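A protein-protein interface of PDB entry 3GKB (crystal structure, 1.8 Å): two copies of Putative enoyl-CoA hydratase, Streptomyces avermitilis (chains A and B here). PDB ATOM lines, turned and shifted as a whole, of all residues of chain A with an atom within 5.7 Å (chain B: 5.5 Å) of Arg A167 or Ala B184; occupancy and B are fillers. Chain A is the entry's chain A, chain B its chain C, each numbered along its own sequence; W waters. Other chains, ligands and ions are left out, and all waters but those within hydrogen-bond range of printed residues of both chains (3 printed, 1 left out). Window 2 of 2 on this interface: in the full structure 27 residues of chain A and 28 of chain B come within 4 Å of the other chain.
The guanidinium group (NH2) of Arg A165 lies within salt-bridge range of the side-chain carboxylate (OD1) of Asp B129 (3.1 Å).
O of Asp B129 is in hydrogen-bond range of ND2 of Asn A166 (2.8 Å).
The side-chain amide nitrogen (ND2) of Asn B190 is in hydrogen-bond range of the backbone carbonyl oxygen (O) of Asn A166 (3.3 Å).
The guanidinium group (NH2) of Arg A167 is in hydrogen-bond range of the backbone carbonyl oxygen (O) of Ala B184, at 2.8 Å.
The backbone carbonyl oxygen (O) of Ile B189 lies within hydrogen-bond range of the guanidinium group (NH2) of Arg A167, at 3.3 Å.
NH2 of Arg A167 sits at hydrogen-bond distance from O of Asn B190 (2.9 Å).
The side-chain amide nitrogen of Asn B190 is in hydrogen-bond range of the side-chain carboxylate of Glu A170, 3.0 Å away.
OE2 of Glu A170 is in salt-bridge range of NH2 of Arg B191 (2.8 Å).
OH of Tyr A186 sits at hydrogen-bond distance from O of Asn B190 (3.2 Å).
The guanidinium group (NE) of Arg B191 lies within hydrogen-bond range of the side-chain hydroxyl (OH) of Tyr A186, 2.8 Å away.
OE1 of Glu A170 lies within hydrogen-bond range of OH of Tyr A186 (2.6 Å).
CA of Gly B187 touches NH1 of Arg A167, at 3.9 Å.
Leu A169 touches Asp B129 (CD1 to CG, 3.999 Å).
Of the printed residues of chain B, Arg A165 touches Asp B129 (3.1 Å).
Of the printed residues of chain B, Arg A167 touches Ala B184, Gly B187, Ile B189 and Asn B190.
Of the printed residues of chain B, Tyr A186 touches Asn B190 (3.2 Å) and Arg B191 (2.8 Å).
Of the printed residues of chain A, Asp B129 touches Arg A165, Asn A166 and Leu A169.
Ala B184 touches just one residue of chain A: Arg A167.
Of the printed residues of chain A, Asn B190 touches Asn A166 (3.3 Å), Arg A167 (2.9 Å), Glu A170 (3.0 Å) and Tyr A186 (3.2 Å).
The nearest residue of chain B that does not touch Arg A167 is Arg B191 (4.6 Å).
The nearest printed residue of chain A that does not touch Ala B184 is Ser A185 (5.9 Å).
The nearest printed residue of chain A that does not touch Asp B129 is Arg A167 (5.0 Å).
Printed residues of chain A that touch a printed residue of chain B: Arg A165, Asn A166, Arg A167, Leu A169, Glu A170 and Tyr A186.
Hydrophobic or aromatic side chains of chain A that line the printed part of chain B: Leu A169 and Tyr A186.
Along chain A the printed residues that touch a printed residue of chain B span positions 165 to 186.
Of the 15 printed residues of chain B, 6 touch a printed residue of chain A.
Among the printed residues, 12 pairs touch across the chains.
Among the printed residues, Asp or Glu carboxylates within 4 Å of a Lys or Arg side-chain nitrogen of the other chain: Arg A165 with Asp B129 and Glu A170 with Arg B191.
Positions printed for both chains: 185 and 186.
Of the 12 pairs that touch across the chains among the printed residues, none has its exchanged pair printed and touching as well.
Water W3 bridges OE2 of Glu A170 (2.6 Å) and NH2 of Arg B191 (3.5 Å).
Water W2 bridges the side-chain carboxylate of Asp B129 and the guanidinium group of Arg A165.
Water W1 bridges the backbone carbonyl oxygen of Ala B184 (3.2 Å) and the guanidinium group of Arg A167 (3.3 Å).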
ATOM      1  N   LEU A 159     -21.400  34.275  -9.997  1.00  0.00           N
ATOM      2  CA  LEU A 159     -21.409  33.720 -11.356  1.00  0.00           C
ATOM      3  C   LEU A 159     -21.286  32.191 -11.290  1.00  0.00           C
ATOM      4  O   LEU A 159     -22.026  31.469 -11.974  1.00  0.00           O
ATOM      5  CB  LEU A 159     -20.272  34.309 -12.205  1.00  0.00           C
ATOM      6  CG  LEU A 159     -20.467  35.705 -12.798  1.00  0.00           C
ATOM      7  CD1 LEU A 159     -19.066  36.332 -13.101  1.00  0.00           C
ATOM      8  CD2 LEU A 159     -21.398  35.656 -14.067  1.00  0.00           C
ATOM      9  N   VAL A 163     -24.331  30.718 -13.277  1.00  0.00           N
ATOM     10  CA  VAL A 163     -24.068  30.374 -14.679  1.00  0.00           C
ATOM     11  C   VAL A 163     -23.195  29.145 -14.844  1.00  0.00           C
ATOM     12  O   VAL A 163     -23.074  28.648 -15.963  1.00  0.00           O
ATOM     13  CB  VAL A 163     -23.501  31.557 -15.475  1.00  0.00           C
ATOM     14  CG1 VAL A 163     -24.357  32.865 -15.272  1.00  0.00           C
ATOM     15  CG2 VAL A 163     -22.021  31.838 -15.151  1.00  0.00           C
ATOM     16  N   GLY A 164     -22.617  28.641 -13.755  1.00  0.00           N
ATOM     17  CA  GLY A 164     -21.648  27.537 -13.811  1.00  0.00           C
ATOM     18  C   GLY A 164     -20.218  28.001 -14.041  1.00  0.00           C
ATOM     19  O   GLY A 164     -19.965  29.076 -14.589  1.00  0.00           O
ATOM     20  N   ARG A 165     -19.257  27.183 -13.620  1.00  0.00           N
ATOM     21  CA  ARG A 165     -17.847  27.552 -13.765  1.00  0.00           C
ATOM     22  C   ARG A 165     -17.388  27.884 -15.197  1.00  0.00           C
ATOM     23  O   ARG A 165     -16.605  28.796 -15.370  1.00  0.00           O
ATOM     24  CB  ARG A 165     -16.963  26.453 -13.182  1.00  0.00           C
ATOM     25  CG  ARG A 165     -15.476  26.683 -13.341  1.00  0.00           C
ATOM     26  CD  ARG A 165     -14.661  25.533 -12.744  1.00  0.00           C
ATOM     27  NE  ARG A 165     -13.301  25.592 -13.265  1.00  0.00           N
ATOM     28  CZ  ARG A 165     -12.935  25.147 -14.466  1.00  0.00           C
ATOM     29  NH1 ARG A 165     -13.813  24.585 -15.296  1.00  0.00           N
ATOM     30  NH2 ARG A 165     -11.687  25.275 -14.856  1.00  0.00           N
ATOM     31  N   ASN A 166     -17.854  27.138 -16.206  1.00  0.00           N
ATOM     32  CA  ASN A 166     -17.408  27.366 -17.579  1.00  0.00           C
ATOM     33  C   ASN A 166     -17.789  28.761 -18.077  1.00  0.00           C
ATOM     34  O   ASN A 166     -16.933  29.510 -18.557  1.00  0.00           O
ATOM     35  CB  ASN A 166     -17.951  26.289 -18.512  1.00  0.00           C
ATOM     36  CG  ASN A 166     -17.450  24.915 -18.140  1.00  0.00           C
ATOM     37  OD1 ASN A 166     -18.183  24.102 -17.550  1.00  0.00           O
ATOM     38  ND2 ASN A 166     -16.181  24.624 -18.505  1.00  0.00           N
ATOM     39  N   ARG A 167     -19.058  29.110 -17.922  1.00  0.00           N
ATOM     40  CA  ARG A 167     -19.505  30.433 -18.274  1.00  0.00           C
ATOM     41  C   ARG A 167     -18.950  31.500 -17.334  1.00  0.00           C
ATOM     42  O   ARG A 167     -18.756  32.651 -17.760  1.00  0.00           O
ATOM     43  CB  ARG A 167     -21.033  30.478 -18.403  1.00  0.00           C
ATOM     44  CG  ARG A 167     -21.480  29.772 -19.671  1.00  0.00           C
ATOM     45  CD  ARG A 167     -22.959  29.525 -19.707  1.00  0.00           C
ATOM     46  NE  ARG A 167     -23.396  29.212 -21.061  1.00  0.00           N
ATOM     47  CZ  ARG A 167     -24.592  28.717 -21.390  1.00  0.00           C
ATOM     48  NH1 ARG A 167     -25.505  28.469 -20.458  1.00  0.00           N
ATOM     49  NH2 ARG A 167     -24.892  28.516 -22.676  1.00  0.00           N
ATOM     50  N   ALA A 168     -18.683  31.156 -16.066  1.00  0.00           N
ATOM     51  CA  ALA A 168     -18.137  32.127 -15.122  1.00  0.00           C
ATOM     52  C   ALA A 168     -16.719  32.539 -15.529  1.00  0.00           C
ATOM     53  O   ALA A 168     -16.394  33.717 -15.544  1.00  0.00           O
ATOM     54  CB  ALA A 168     -18.157  31.587 -13.695  1.00  0.00           C
ATOM     55  N   LEU A 169     -15.907  31.563 -15.947  1.00  0.00           N
ATOM     56  CA  LEU A 169     -14.569  31.853 -16.450  1.00  0.00           C
ATOM     57  C   LEU A 169     -14.609  32.714 -17.728  1.00  0.00           C
ATOM     58  O   LEU A 169     -13.823  33.633 -17.879  1.00  0.00           O
ATOM     59  CB  LEU A 169     -13.791  30.555 -16.738  1.00  0.00           C
ATOM     60  CG  LEU A 169     -13.198  29.884 -15.512  1.00  0.00           C
ATOM     61  CD1 LEU A 169     -12.721  28.476 -15.846  1.00  0.00           C
ATOM     62  CD2 LEU A 169     -12.077  30.761 -14.954  1.00  0.00           C
ATOM     63  N   GLU A 170     -15.548  32.401 -18.621  1.00  0.00           N
ATOM     64  CA  GLU A 170     -15.782  33.175 -19.818  1.00  0.00           C
ATOM     65  C   GLU A 170     -16.123  34.632 -19.464  1.00  0.00           C
ATOM     66  O   GLU A 170     -15.513  35.551 -19.971  1.00  0.00           O
ATOM     67  CB  GLU A 170     -16.905  32.559 -20.655  1.00  0.00           C
ATOM     68  CG  GLU A 170     -17.153  33.313 -21.984  1.00  0.00           C
ATOM     69  CD  GLU A 170     -18.488  32.989 -22.620  1.00  0.00           C
ATOM     70  OE1 GLU A 170     -19.185  32.044 -22.179  1.00  0.00           O
ATOM     71  OE2 GLU A 170     -18.831  33.727 -23.559  1.00  0.00           O
ATOM     72  N   VAL A 171     -17.067  34.828 -18.575  1.00  0.00           N
ATOM     73  CA  VAL A 171     -17.475  36.211 -18.219  1.00  0.00           C
ATOM     74  C   VAL A 171     -16.311  36.960 -17.606  1.00  0.00           C
ATOM     75  O   VAL A 171     -16.019  38.101 -17.992  1.00  0.00           O
ATOM     76  CB  VAL A 171     -18.667  36.202 -17.255  1.00  0.00           C
ATOM     77  CG1 VAL A 171     -18.914  37.577 -16.668  1.00  0.00           C
ATOM     78  CG2 VAL A 171     -19.926  35.717 -17.949  1.00  0.00           C
ATOM     79  N   VAL A 172     -15.607  36.308 -16.689  1.00  0.00           N
ATOM     80  CA  VAL A 172     -14.508  36.964 -15.955  1.00  0.00           C
ATOM     81  C   VAL A 172     -13.326  37.288 -16.867  1.00  0.00           C
ATOM     82  O   VAL A 172     -12.782  38.392 -16.802  1.00  0.00           O
ATOM     83  CB  VAL A 172     -14.096  36.148 -14.714  1.00  0.00           C
ATOM     84  CG1 VAL A 172     -12.700  36.609 -14.106  1.00  0.00           C
ATOM     85  CG2 VAL A 172     -15.230  36.216 -13.701  1.00  0.00           C
ATOM     86  N   SER A 185     -30.038  34.087 -20.818  1.00  0.00           N
ATOM     87  CA  SER A 185     -29.804  32.721 -21.281  1.00  0.00           C
ATOM     88  C   SER A 185     -28.823  31.982 -20.379  1.00  0.00           C
ATOM     89  O   SER A 185     -28.995  30.806 -20.074  1.00  0.00           O
ATOM     90  CB  SER A 185     -29.278  32.746 -22.710  1.00  0.00           C
ATOM     91  OG  SER A 185     -30.139  33.535 -23.511  1.00  0.00           O
ATOM     92  N   TYR A 186     -27.780  32.689 -19.954  1.00  0.00           N
ATOM     93  CA  TYR A 186     -26.751  32.134 -19.063  1.00  0.00           C
ATOM     94  C   TYR A 186     -27.267  31.869 -17.639  1.00  0.00           C
ATOM     95  O   TYR A 186     -26.724  31.017 -16.918  1.00  0.00           O
ATOM     96  CB  TYR A 186     -25.547  33.081 -18.999  1.00  0.00           C
ATOM     97  CG  TYR A 186     -24.510  32.921 -20.102  1.00  0.00           C
ATOM     98  CD1 TYR A 186     -24.843  32.414 -21.354  1.00  0.00           C
ATOM     99  CD2 TYR A 186     -23.198  33.241 -19.861  1.00  0.00           C
ATOM    100  CE1 TYR A 186     -23.877  32.265 -22.346  1.00  0.00           C
ATOM    101  CE2 TYR A 186     -22.206  33.098 -20.832  1.00  0.00           C
ATOM    102  CZ  TYR A 186     -22.570  32.610 -22.090  1.00  0.00           C
ATOM    103  OH  TYR A 186     -21.619  32.438 -23.056  1.00  0.00           O
ATOM    104  N   ASP B 129     -12.375  24.678 -20.581  1.00  0.00           N
ATOM    105  CA  ASP B 129     -12.936  25.836 -19.859  1.00  0.00           C
ATOM    106  C   ASP B 129     -14.124  26.460 -20.615  1.00  0.00           C
ATOM    107  O   ASP B 129     -15.161  26.803 -20.014  1.00  0.00           O
ATOM    108  CB  ASP B 129     -11.889  26.888 -19.581  1.00  0.00           C
ATOM    109  CG  ASP B 129     -10.792  26.393 -18.662  1.00  0.00           C
ATOM    110  OD1 ASP B 129     -11.006  25.433 -17.863  1.00  0.00           O
ATOM    111  OD2 ASP B 129      -9.695  26.968 -18.754  1.00  0.00           O
ATOM    112  N   ASP B 179     -27.927  19.705 -31.848  1.00  0.00           N
ATOM    113  CA  ASP B 179     -27.399  20.825 -32.586  1.00  0.00           C
ATOM    114  C   ASP B 179     -26.792  21.843 -31.622  1.00  0.00           C
ATOM    115  O   ASP B 179     -26.950  21.725 -30.417  1.00  0.00           O
ATOM    116  CB  ASP B 179     -28.414  21.466 -33.575  1.00  0.00           C
ATOM    117  CG  ASP B 179     -29.635  22.086 -32.903  1.00  0.00           C
ATOM    118  OD1 ASP B 179     -29.588  22.565 -31.759  1.00  0.00           O
ATOM    119  OD2 ASP B 179     -30.697  22.090 -33.571  1.00  0.00           O
ATOM    120  N   ALA B 180     -26.062  22.814 -32.163  1.00  0.00           N
ATOM    121  CA  ALA B 180     -25.372  23.822 -31.355  1.00  0.00           C
ATOM    122  C   ALA B 180     -26.277  24.710 -30.522  1.00  0.00           C
ATOM    123  O   ALA B 180     -25.989  24.970 -29.334  1.00  0.00           O
ATOM    124  CB  ALA B 180     -24.401  24.669 -32.246  1.00  0.00           C
ATOM    125  N   GLU B 181     -27.401  25.156 -31.105  1.00  0.00           N
ATOM    126  CA  GLU B 181     -28.331  25.986 -30.372  1.00  0.00           C
ATOM    127  C   GLU B 181     -28.885  25.260 -29.145  1.00  0.00           C
ATOM    128  O   GLU B 181     -28.994  25.859 -28.061  1.00  0.00           O
ATOM    129  CB  GLU B 181     -29.486  26.471 -31.283  1.00  0.00           C
ATOM    130  N   THR B 182     -29.237  23.989 -29.312  1.00  0.00           N
ATOM    131  CA  THR B 182     -29.769  23.184 -28.197  1.00  0.00           C
ATOM    132  C   THR B 182     -28.722  22.892 -27.154  1.00  0.00           C
ATOM    133  O   THR B 182     -28.991  22.993 -25.955  1.00  0.00           O
ATOM    134  CB  THR B 182     -30.382  21.865 -28.669  1.00  0.00           C
ATOM    135  OG1 THR B 182     -31.293  22.131 -29.744  1.00  0.00           O
ATOM    136  CG2 THR B 182     -31.112  21.186 -27.494  1.00  0.00           C
ATOM    137  N   ALA B 183     -27.510  22.564 -27.612  1.00  0.00           N
ATOM    138  CA  ALA B 183     -26.405  22.315 -26.685  1.00  0.00           C
ATOM    139  C   ALA B 183     -26.125  23.565 -25.846  1.00  0.00           C
ATOM    140  O   ALA B 183     -25.928  23.471 -24.623  1.00  0.00           O
ATOM    141  CB  ALA B 183     -25.143  21.882 -27.418  1.00  0.00           C
ATOM    142  N   ALA B 184     -26.087  24.735 -26.497  1.00  0.00           N
ATOM    143  CA  ALA B 184     -25.865  25.986 -25.764  1.00  0.00           C
ATOM    144  C   ALA B 184     -27.013  26.280 -24.793  1.00  0.00           C
ATOM    145  O   ALA B 184     -26.770  26.706 -23.674  1.00  0.00           O
ATOM    146  CB  ALA B 184     -25.650  27.158 -26.721  1.00  0.00           C
ATOM    147  N   SER B 185     -28.261  26.089 -25.207  1.00  0.00           N
ATOM    148  CA  SER B 185     -29.400  26.340 -24.312  1.00  0.00           C
ATOM    149  C   SER B 185     -29.312  25.456 -23.080  1.00  0.00           C
ATOM    150  O   SER B 185     -29.634  25.885 -21.977  1.00  0.00           O
ATOM    151  CB  SER B 185     -30.727  26.088 -25.019  1.00  0.00           C
ATOM    152  OG  SER B 185     -30.898  27.002 -26.080  1.00  0.00           O
ATOM    153  N   TYR B 186     -28.840  24.223 -23.275  1.00  0.00           N
ATOM    154  CA  TYR B 186     -28.692  23.272 -22.176  1.00  0.00           C
ATOM    155  C   TYR B 186     -27.517  23.630 -21.261  1.00  0.00           C
ATOM    156  O   TYR B 186     -27.517  23.244 -20.104  1.00  0.00           O
ATOM    157  CB  TYR B 186     -28.509  21.855 -22.706  1.00  0.00           C
ATOM    158  CG  TYR B 186     -29.781  21.096 -23.058  1.00  0.00           C
ATOM    159  CD1 TYR B 186     -30.948  21.757 -23.435  1.00  0.00           C
ATOM    160  CD2 TYR B 186     -29.799  19.725 -23.025  1.00  0.00           C
ATOM    161  CE1 TYR B 186     -32.092  21.070 -23.757  1.00  0.00           C
ATOM    162  CE2 TYR B 186     -30.921  19.008 -23.315  1.00  0.00           C
ATOM    163  CZ  TYR B 186     -32.083  19.673 -23.689  1.00  0.00           C
ATOM    164  OH  TYR B 186     -33.210  18.962 -23.990  1.00  0.00           O
ATOM    165  N   GLY B 187     -26.534  24.369 -21.778  1.00  0.00           N
ATOM    166  CA  GLY B 187     -25.297  24.660 -21.041  1.00  0.00           C
ATOM    167  C   GLY B 187     -24.147  23.709 -21.322  1.00  0.00           C
ATOM    168  O   GLY B 187     -23.123  23.755 -20.628  1.00  0.00           O
ATOM    169  N   TRP B 188     -24.320  22.825 -22.301  1.00  0.00           N
ATOM    170  CA  TRP B 188     -23.307  21.778 -22.608  1.00  0.00           C
ATOM    171  C   TRP B 188     -22.060  22.454 -23.230  1.00  0.00           C
ATOM    172  O   TRP B 188     -20.941  21.984 -23.038  1.00  0.00           O
ATOM    173  CB  TRP B 188     -23.916  20.794 -23.595  1.00  0.00           C
ATOM    174  CG  TRP B 188     -23.241  19.482 -23.768  1.00  0.00           C
ATOM    175  CD1 TRP B 188     -22.085  19.070 -23.210  1.00  0.00           C
ATOM    176  CD2 TRP B 188     -23.692  18.408 -24.612  1.00  0.00           C
ATOM    177  NE1 TRP B 188     -21.787  17.785 -23.626  1.00  0.00           N
ATOM    178  CE2 TRP B 188     -22.752  17.363 -24.497  1.00  0.00           C
ATOM    179  CE3 TRP B 188     -24.828  18.210 -25.405  1.00  0.00           C
ATOM    180  CZ2 TRP B 188     -22.908  16.130 -25.155  1.00  0.00           C
ATOM    181  CZ3 TRP B 188     -24.961  17.001 -26.082  1.00  0.00           C
ATOM    182  CH2 TRP B 188     -24.014  15.983 -25.941  1.00  0.00           C
ATOM    183  N   ILE B 189     -22.283  23.550 -23.969  1.00  0.00           N
ATOM    184  CA  ILE B 189     -21.229  24.463 -24.489  1.00  0.00           C
ATOM    185  C   ILE B 189     -21.574  25.875 -24.018  1.00  0.00           C
ATOM    186  O   ILE B 189     -22.700  26.128 -23.509  1.00  0.00           O
ATOM    187  CB  ILE B 189     -21.117  24.435 -26.055  1.00  0.00           C
ATOM    188  CG1 ILE B 189     -22.447  24.782 -26.720  1.00  0.00           C
ATOM    189  CG2 ILE B 189     -20.643  23.043 -26.502  1.00  0.00           C
ATOM    190  CD1 ILE B 189     -22.405  24.997 -28.242  1.00  0.00           C
ATOM    191  N   ASN B 190     -20.627  26.794 -24.179  1.00  0.00           N
ATOM    192  CA  ASN B 190     -20.822  28.166 -23.728  1.00  0.00           C
ATOM    193  C   ASN B 190     -21.788  28.930 -24.646  1.00  0.00           C
ATOM    194  O   ASN B 190     -22.674  29.596 -24.166  1.00  0.00           O
ATOM    195  CB  ASN B 190     -19.496  28.934 -23.607  1.00  0.00           C
ATOM    196  CG  ASN B 190     -18.615  28.422 -22.515  1.00  0.00           C
ATOM    197  OD1 ASN B 190     -18.256  27.246 -22.492  1.00  0.00           O
ATOM    198  ND2 ASN B 190     -18.246  29.308 -21.576  1.00  0.00           N
ATOM    199  N   ARG B 191     -21.621  28.814 -25.962  1.00  0.00           N
ATOM    200  CA  ARG B 191     -22.340  29.641 -26.912  1.00  0.00           C
ATOM    201  C   ARG B 191     -22.346  29.010 -28.296  1.00  0.00           C
ATOM    202  O   ARG B 191     -21.360  28.384 -28.690  1.00  0.00           O
ATOM    203  CB  ARG B 191     -21.692  31.019 -26.991  1.00  0.00           C
ATOM    204  CG  ARG B 191     -22.635  32.115 -27.485  1.00  0.00           C
ATOM    205  CD  ARG B 191     -23.356  32.767 -26.346  1.00  0.00           C
ATOM    206  NE  ARG B 191     -22.342  33.454 -25.544  1.00  0.00           N
ATOM    207  CZ  ARG B 191     -21.819  34.649 -25.780  1.00  0.00           C
ATOM    208  NH1 ARG B 191     -22.272  35.442 -26.751  1.00  0.00           N
ATOM    209  NH2 ARG B 191     -20.835  35.072 -24.972  1.00  0.00           N
ATOM    210  N   ALA B 192     -23.448  29.203 -29.023  1.00  0.00           N
ATOM    211  CA  ALA B 192     -23.513  28.916 -30.443  1.00  0.00           C
ATOM    212  C   ALA B 192     -23.399  30.233 -31.223  1.00  0.00           C
ATOM    213  O   ALA B 192     -24.030  31.241 -30.870  1.00  0.00           O
ATOM    214  CB  ALA B 192     -24.804  28.176 -30.799  1.00  0.00           C
HETATM  215  O   HOH W   1     -27.808  29.711 -23.793  1.00  0.00           O
HETATM  216  O   HOH W   2     -12.596  23.163 -17.611  1.00  0.00           O
HETATM  217  O   HOH W   3     -17.363  35.012 -25.275  1.00  0.00           O
